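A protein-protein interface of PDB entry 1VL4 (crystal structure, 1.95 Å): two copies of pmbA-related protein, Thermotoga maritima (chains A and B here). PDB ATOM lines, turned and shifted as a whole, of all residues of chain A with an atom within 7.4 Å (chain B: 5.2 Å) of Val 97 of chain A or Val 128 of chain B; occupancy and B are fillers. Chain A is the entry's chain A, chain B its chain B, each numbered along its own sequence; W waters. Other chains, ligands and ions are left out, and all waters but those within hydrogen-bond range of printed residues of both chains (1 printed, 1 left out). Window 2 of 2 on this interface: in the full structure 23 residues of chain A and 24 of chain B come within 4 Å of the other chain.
OG of Ser 127 of chain B lies close to N of Lys 129 of chain B (3.4 Å). NZ of Lys 129 of chain B lies within salt-bridge range of OD2 of Asp 133 of chain B, 2.6 Å away. The side-chain amide nitrogen (NE2) of Gln 96 of chain A sits at hydrogen-bond distance from the backbone carbonyl oxygen (O) of Ser 93 of chain A, at 2.9 Å.
Tyr 55 of chain B touches Gly 74 of chain A (OH to CA, 3.4 Å). CG2 of Val 128 of chain B touches OG of Ser 93 of chain A (3.9 Å). Asn 94 of chain A touches Phe 43 of chain B (OD1 to CE1, 3.9 Å). CB of Asn 94 of chain A touches OH of Tyr 55 of chain B (3.6 Å). Asn 94 of chain A touches Val 128 of chain B (OD1 to CG2, 3.6 Å). OE1 of Gln 96 of chain A touches CB of Lys 129 of chain B, 3.5 Å away. CG1 of Val 97 of chain A touches CD1 of Tyr 55 of chain B (3.8 Å). Val 128 of chain B touches Val 97 of chain A (CG1 to CG2, 3.5 Å). Leu 52 of chain B touches Lys 98 of chain A (N to NZ, 3.6 Å).
Water W1 bridges the side-chain hydroxyl of Tyr 55 of chain B (2.7 Å) and the side-chain hydroxyl of Thr 73 of chain A (3.0 Å).
Of the printed residues of chain B, Val 97 of chain A touches Tyr 55 and Val 128. Printed residues of chain B within 4 Å of Gly 74 of chain A: Tyr 55. Printed residues of chain A within 4 Å of Leu 52 of chain B: Lys 98. Of the printed residues of chain B, Ser 93 of chain A touches Val 128 (3.9 Å). Glu 130 of chain B touches none of the printed residues of chain A. Ala 91 of chain A touches none of the printed residues of chain B. The nearest printed residue of chain B that does not touch Val 97 of chain A is Met 132 of chain B (4.2 Å). The nearest residue of chain A that does not touch Val 128 of chain B is Gln 96 of chain A (4.3 Å). The nearest printed residue of chain A that does not touch Lys 129 of chain B is Ser 93 of chain A (6.4 Å).
No position is printed for both chains.
Of the 11 printed residues of chain B, 5 touch a printed residue of chain A. Among the printed residues, no Asp or Glu carboxylate lies within 4 Å of a Lys or Arg side-chain nitrogen of the other chain.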
ATOM      1  N   LYS A  72      -0.010  -5.307   4.858  1.00  0.00           N
ATOM      2  CA  LYS A  72      -0.636  -5.296   3.551  1.00  0.00           C
ATOM      3  C   LYS A  72      -1.593  -4.101   3.492  1.00  0.00           C
ATOM      4  O   LYS A  72      -2.222  -3.773   4.515  1.00  0.00           O
ATOM      5  CB  LYS A  72      -1.417  -6.574   3.348  1.00  0.00           C
ATOM      6  CG  LYS A  72      -0.584  -7.756   2.939  1.00  0.00           C
ATOM      7  CD  LYS A  72      -1.472  -8.956   2.752  1.00  0.00           C
ATOM      8  CE  LYS A  72      -0.748 -10.234   3.182  1.00  0.00           C
ATOM      9  NZ  LYS A  72      -1.461 -11.423   2.661  1.00  0.00           N
ATOM     10  N   THR A  73      -1.654  -3.436   2.320  1.00  0.00           N
ATOM     11  CA  THR A  73      -2.635  -2.357   2.045  1.00  0.00           C
ATOM     12  C   THR A  73      -3.760  -2.716   1.037  1.00  0.00           C
ATOM     13  O   THR A  73      -3.666  -3.654   0.238  1.00  0.00           O
ATOM     14  CB  THR A  73      -1.978  -1.113   1.610  1.00  0.00           C
ATOM     15  OG1 THR A  73      -1.227  -1.334   0.404  1.00  0.00           O
ATOM     16  CG2 THR A  73      -1.052  -0.616   2.660  1.00  0.00           C
ATOM     17  N   GLY A  74      -4.876  -2.019   1.199  1.00  0.00           N
ATOM     18  CA  GLY A  74      -6.057  -2.129   0.325  1.00  0.00           C
ATOM     19  C   GLY A  74      -6.457  -0.681   0.096  1.00  0.00           C
ATOM     20  O   GLY A  74      -6.479   0.120   1.043  1.00  0.00           O
ATOM     21  N   GLU A  90     -14.748  -1.535   0.556  1.00  0.00           N
ATOM     22  CA  GLU A  90     -14.090  -1.692  -0.739  1.00  0.00           C
ATOM     23  C   GLU A  90     -12.579  -1.764  -0.564  1.00  0.00           C
ATOM     24  O   GLU A  90     -11.916  -2.644  -1.108  1.00  0.00           O
ATOM     25  CB  GLU A  90     -14.491  -0.533  -1.647  1.00  0.00           C
ATOM     26  CG  GLU A  90     -14.057  -0.668  -3.084  1.00  0.00           C
ATOM     27  CD  GLU A  90     -14.788  -1.755  -3.885  1.00  0.00           C
ATOM     28  OE1 GLU A  90     -15.716  -2.436  -3.404  1.00  0.00           O
ATOM     29  OE2 GLU A  90     -14.369  -1.952  -5.022  1.00  0.00           O
ATOM     30  N   ALA A  91     -12.018  -0.871   0.243  1.00  0.00           N
ATOM     31  CA  ALA A  91     -10.549  -0.846   0.483  1.00  0.00           C
ATOM     32  C   ALA A  91     -10.138  -2.124   1.198  1.00  0.00           C
ATOM     33  O   ALA A  91      -9.100  -2.712   0.889  1.00  0.00           O
ATOM     34  CB  ALA A  91     -10.152   0.348   1.309  1.00  0.00           C
ATOM     35  N   LEU A  92     -10.951  -2.549   2.157  1.00  0.00           N
ATOM     36  CA  LEU A  92     -10.655  -3.745   2.929  1.00  0.00           C
ATOM     37  C   LEU A  92     -10.616  -4.956   1.979  1.00  0.00           C
ATOM     38  O   LEU A  92      -9.699  -5.805   2.004  1.00  0.00           O
ATOM     39  CB  LEU A  92     -11.746  -3.922   3.991  1.00  0.00           C
ATOM     40  CG  LEU A  92     -11.389  -4.773   5.207  1.00  0.00           C
ATOM     41  CD1 LEU A  92     -10.368  -4.071   6.062  1.00  0.00           C
ATOM     42  CD2 LEU A  92     -12.667  -5.123   6.019  1.00  0.00           C
ATOM     43  N   SER A  93     -11.595  -5.016   1.081  1.00  0.00           N
ATOM     44  CA  SER A  93     -11.641  -6.124   0.179  1.00  0.00           C
ATOM     45  C   SER A  93     -10.396  -6.182  -0.724  1.00  0.00           C
ATOM     46  O   SER A  93      -9.950  -7.255  -1.080  1.00  0.00           O
ATOM     47  CB  SER A  93     -12.970  -6.162  -0.606  1.00  0.00           C
ATOM     48  OG  SER A  93     -12.816  -6.966  -1.748  1.00  0.00           O
ATOM     49  N   ASN A  94      -9.813  -5.056  -1.073  1.00  0.00           N
ATOM     50  CA  ASN A  94      -8.600  -5.050  -1.853  1.00  0.00           C
ATOM     51  C   ASN A  94      -7.319  -5.469  -1.123  1.00  0.00           C
ATOM     52  O   ASN A  94      -6.245  -5.533  -1.741  1.00  0.00           O
ATOM     53  CB  ASN A  94      -8.398  -3.688  -2.506  1.00  0.00           C
ATOM     54  CG  ASN A  94      -9.496  -3.370  -3.564  1.00  0.00           C
ATOM     55  OD1 ASN A  94     -10.151  -4.259  -4.085  1.00  0.00           O
ATOM     56  ND2 ASN A  94      -9.659  -2.094  -3.862  1.00  0.00           N
ATOM     57  N   LEU A  95      -7.406  -5.713   0.183  1.00  0.00           N
ATOM     58  CA  LEU A  95      -6.247  -6.255   0.917  1.00  0.00           C
ATOM     59  C   LEU A  95      -5.766  -7.576   0.332  1.00  0.00           C
ATOM     60  O   LEU A  95      -4.592  -7.836   0.331  1.00  0.00           O
ATOM     61  CB  LEU A  95      -6.560  -6.479   2.394  1.00  0.00           C
ATOM     62  CG  LEU A  95      -6.442  -5.235   3.271  1.00  0.00           C
ATOM     63  CD1 LEU A  95      -6.926  -5.615   4.681  1.00  0.00           C
ATOM     64  CD2 LEU A  95      -5.045  -4.649   3.321  1.00  0.00           C
ATOM     65  N   GLN A  96      -6.674  -8.385  -0.174  1.00  0.00           N
ATOM     66  CA  GLN A  96      -6.316  -9.661  -0.809  1.00  0.00           C
ATOM     67  C   GLN A  96      -5.589  -9.583  -2.174  1.00  0.00           C
ATOM     68  O   GLN A  96      -5.170 -10.602  -2.716  1.00  0.00           O
ATOM     69  CB  GLN A  96      -7.590 -10.486  -0.976  1.00  0.00           C
ATOM     70  CG  GLN A  96      -8.510  -9.869  -1.988  1.00  0.00           C
ATOM     71  CD  GLN A  96      -9.808 -10.556  -2.113  1.00  0.00           C
ATOM     72  OE1 GLN A  96      -9.887 -11.646  -2.670  1.00  0.00           O
ATOM     73  NE2 GLN A  96     -10.863  -9.914  -1.638  1.00  0.00           N
ATOM     74  N   VAL A  97      -5.471  -8.401  -2.762  1.00  0.00           N
ATOM     75  CA  VAL A  97      -4.865  -8.261  -4.106  1.00  0.00           C
ATOM     76  C   VAL A  97      -3.329  -8.408  -3.947  1.00  0.00           C
ATOM     77  O   VAL A  97      -2.538  -7.495  -4.239  1.00  0.00           O
ATOM     78  CB  VAL A  97      -5.326  -6.908  -4.768  1.00  0.00           C
ATOM     79  CG1 VAL A  97      -4.793  -6.767  -6.177  1.00  0.00           C
ATOM     80  CG2 VAL A  97      -6.855  -6.834  -4.788  1.00  0.00           C
ATOM     81  N   LYS A  98      -2.939  -9.598  -3.457  1.00  0.00           N
ATOM     82  CA  LYS A  98      -1.661  -9.873  -2.692  1.00  0.00           C
ATOM     83  C   LYS A  98      -1.898  -9.718  -1.172  1.00  0.00           C
ATOM     84  O   LYS A  98      -2.033  -8.602  -0.650  1.00  0.00           O
ATOM     85  CB  LYS A  98      -0.429  -9.050  -3.164  1.00  0.00           C
ATOM     86  CG  LYS A  98       0.710  -9.884  -3.793  1.00  0.00           C
ATOM     87  CD  LYS A  98       0.240 -10.525  -5.099  1.00  0.00           C
ATOM     88  CE  LYS A  98       1.271 -11.455  -5.721  1.00  0.00           C
ATOM     89  NZ  LYS A  98       0.607 -12.436  -6.636  1.00  0.00           N
ATOM     90  N   PHE B  43     -11.828  -0.797 -12.427  1.00  0.00           N
ATOM     91  CA  PHE B  43     -10.992  -1.642 -11.631  1.00  0.00           C
ATOM     92  C   PHE B  43     -10.015  -2.199 -12.607  1.00  0.00           C
ATOM     93  O   PHE B  43     -10.432  -2.705 -13.661  1.00  0.00           O
ATOM     94  CB  PHE B  43     -11.771  -2.790 -10.993  1.00  0.00           C
ATOM     95  CG  PHE B  43     -10.900  -3.678 -10.138  1.00  0.00           C
ATOM     96  CD1 PHE B  43     -10.652  -3.352  -8.812  1.00  0.00           C
ATOM     97  CD2 PHE B  43     -10.287  -4.788 -10.678  1.00  0.00           C
ATOM     98  CE1 PHE B  43      -9.830  -4.129  -8.019  1.00  0.00           C
ATOM     99  CE2 PHE B  43      -9.456  -5.579  -9.881  1.00  0.00           C
ATOM    100  CZ  PHE B  43      -9.215  -5.227  -8.534  1.00  0.00           C
ATOM    101  N   LEU B  52       1.316  -9.827  -8.986  1.00  0.00           N
ATOM    102  CA  LEU B  52       0.322  -8.809  -9.066  1.00  0.00           C
ATOM    103  C   LEU B  52       0.865  -7.626  -8.318  1.00  0.00           C
ATOM    104  O   LEU B  52       0.882  -7.624  -7.106  1.00  0.00           O
ATOM    105  CB  LEU B  52      -0.991  -9.307  -8.476  1.00  0.00           C
ATOM    106  N   TYR B  55      -2.670  -2.227  -9.176  1.00  0.00           N
ATOM    107  CA  TYR B  55      -4.111  -2.258  -9.390  1.00  0.00           C
ATOM    108  C   TYR B  55      -4.655  -0.853  -9.147  1.00  0.00           C
ATOM    109  O   TYR B  55      -4.040  -0.040  -8.430  1.00  0.00           O
ATOM    110  CB  TYR B  55      -4.789  -3.306  -8.469  1.00  0.00           C
ATOM    111  CG  TYR B  55      -4.907  -2.922  -7.007  1.00  0.00           C
ATOM    112  CD1 TYR B  55      -3.843  -3.127  -6.098  1.00  0.00           C
ATOM    113  CD2 TYR B  55      -6.084  -2.370  -6.523  1.00  0.00           C
ATOM    114  CE1 TYR B  55      -3.959  -2.779  -4.770  1.00  0.00           C
ATOM    115  CE2 TYR B  55      -6.218  -2.038  -5.206  1.00  0.00           C
ATOM    116  CZ  TYR B  55      -5.151  -2.222  -4.336  1.00  0.00           C
ATOM    117  OH  TYR B  55      -5.289  -1.869  -3.028  1.00  0.00           O
ATOM    118  N   LEU B 126     -18.798  -9.504 -10.520  1.00  0.00           N
ATOM    119  CA  LEU B 126     -17.609 -10.296 -10.182  1.00  0.00           C
ATOM    120  C   LEU B 126     -16.969  -9.847  -8.872  1.00  0.00           C
ATOM    121  O   LEU B 126     -16.865  -8.638  -8.614  1.00  0.00           O
ATOM    122  CB  LEU B 126     -16.550 -10.102 -11.263  1.00  0.00           C
ATOM    123  CG  LEU B 126     -16.843 -10.658 -12.650  1.00  0.00           C
ATOM    124  CD1 LEU B 126     -15.627 -10.378 -13.515  1.00  0.00           C
ATOM    125  CD2 LEU B 126     -17.130 -12.146 -12.535  1.00  0.00           C
ATOM    126  N   SER B 127     -16.516 -10.800  -8.083  1.00  0.00           N
ATOM    127  CA  SER B 127     -15.686 -10.490  -6.919  1.00  0.00           C
ATOM    128  C   SER B 127     -14.277 -10.080  -7.336  1.00  0.00           C
ATOM    129  O   SER B 127     -13.844 -10.379  -8.464  1.00  0.00           O
ATOM    130  CB  SER B 127     -15.614 -11.672  -6.025  1.00  0.00           C
ATOM    131  OG  SER B 127     -14.735 -12.628  -6.593  1.00  0.00           O
ATOM    132  N   VAL B 128     -13.526  -9.481  -6.410  1.00  0.00           N
ATOM    133  CA  VAL B 128     -12.145  -9.080  -6.680  1.00  0.00           C
ATOM    134  C   VAL B 128     -11.293 -10.336  -6.908  1.00  0.00           C
ATOM    135  O   VAL B 128     -10.418 -10.353  -7.770  1.00  0.00           O
ATOM    136  CB  VAL B 128     -11.573  -8.170  -5.537  1.00  0.00           C
ATOM    137  CG1 VAL B 128     -10.064  -8.051  -5.602  1.00  0.00           C
ATOM    138  CG2 VAL B 128     -12.205  -6.771  -5.624  1.00  0.00           C
ATOM    139  N   LYS B 129     -11.576 -11.389  -6.155  1.00  0.00           N
ATOM    140  CA  LYS B 129     -10.891 -12.641  -6.315  1.00  0.00           C
ATOM    141  C   LYS B 129     -11.119 -13.248  -7.695  1.00  0.00           C
ATOM    142  O   LYS B 129     -10.208 -13.813  -8.255  1.00  0.00           O
ATOM    143  CB  LYS B 129     -11.283 -13.636  -5.227  1.00  0.00           C
ATOM    144  CG  LYS B 129     -10.553 -14.964  -5.375  1.00  0.00           C
ATOM    145  CD  LYS B 129     -10.714 -15.826  -4.179  1.00  0.00           C
ATOM    146  CE  LYS B 129     -10.045 -17.209  -4.328  1.00  0.00           C
ATOM    147  NZ  LYS B 129     -10.167 -17.779  -5.674  1.00  0.00           N
ATOM    148  N   GLU B 130     -12.332 -13.158  -8.208  1.00  0.00           N
ATOM    149  CA  GLU B 130     -12.632 -13.662  -9.548  1.00  0.00           C
ATOM    150  C   GLU B 130     -11.839 -12.928 -10.639  1.00  0.00           C
ATOM    151  O   GLU B 130     -11.342 -13.569 -11.573  1.00  0.00           O
ATOM    152  CB  GLU B 130     -14.138 -13.591  -9.800  1.00  0.00           C
ATOM    153  CG  GLU B 130     -14.938 -14.674  -9.047  1.00  0.00           C
ATOM    154  CD  GLU B 130     -16.472 -14.470  -9.100  1.00  0.00           C
ATOM    155  OE1 GLU B 130     -16.962 -13.314  -8.999  1.00  0.00           O
ATOM    156  OE2 GLU B 130     -17.188 -15.498  -9.207  1.00  0.00           O
ATOM    157  N   LYS B 131     -11.716 -11.605 -10.511  1.00  0.00           N
ATOM    158  CA  LYS B 131     -10.963 -10.779 -11.467  1.00  0.00           C
ATOM    159  C   LYS B 131      -9.503 -11.164 -11.406  1.00  0.00           C
ATOM    160  O   LYS B 131      -8.840 -11.372 -12.454  1.00  0.00           O
ATOM    161  CB  LYS B 131     -11.154  -9.294 -11.169  1.00  0.00           C
ATOM    162  CG  LYS B 131     -12.588  -8.826 -11.339  1.00  0.00           C
ATOM    163  CD  LYS B 131     -12.848  -7.432 -10.842  1.00  0.00           C
ATOM    164  CE  LYS B 131     -14.308  -7.124 -10.983  1.00  0.00           C
ATOM    165  NZ  LYS B 131     -14.599  -5.660 -10.992  1.00  0.00           N
ATOM    166  N   MET B 132      -9.012 -11.307 -10.170  1.00  0.00           N
ATOM    167  CA  MET B 132      -7.626 -11.738  -9.875  1.00  0.00           C
ATOM    168  C   MET B 132      -7.365 -13.162 -10.429  1.00  0.00           C
ATOM    169  O   MET B 132      -6.269 -13.460 -10.900  1.00  0.00           O
ATOM    170  CB  MET B 132      -7.295 -11.652  -8.340  1.00  0.00           C
ATOM    171  CG  MET B 132      -5.801 -11.735  -8.033  1.00  0.00           C
ATOM    172  SD  MET B 132      -4.861 -10.251  -8.487  1.00  0.00           S
ATOM    173  CE  MET B 132      -3.311 -11.019  -8.864  1.00  0.00           C
ATOM    174  N   ASP B 133      -8.369 -14.040 -10.351  1.00  0.00           N
ATOM    175  CA  ASP B 133      -8.255 -15.413 -10.844  1.00  0.00           C
ATOM    176  C   ASP B 133      -8.249 -15.424 -12.379  1.00  0.00           C
ATOM    177  O   ASP B 133      -7.610 -16.294 -12.981  1.00  0.00           O
ATOM    178  CB  ASP B 133      -9.380 -16.315 -10.309  1.00  0.00           C
ATOM    179  CG  ASP B 133      -9.282 -16.615  -8.782  1.00  0.00           C
ATOM    180  OD1 ASP B 133      -8.234 -16.409  -8.133  1.00  0.00           O
ATOM    181  OD2 ASP B 133     -10.302 -17.080  -8.225  1.00  0.00           O
HETATM  182  O   HOH W   1      -2.894  -1.031  -2.020  1.00  0.00           O
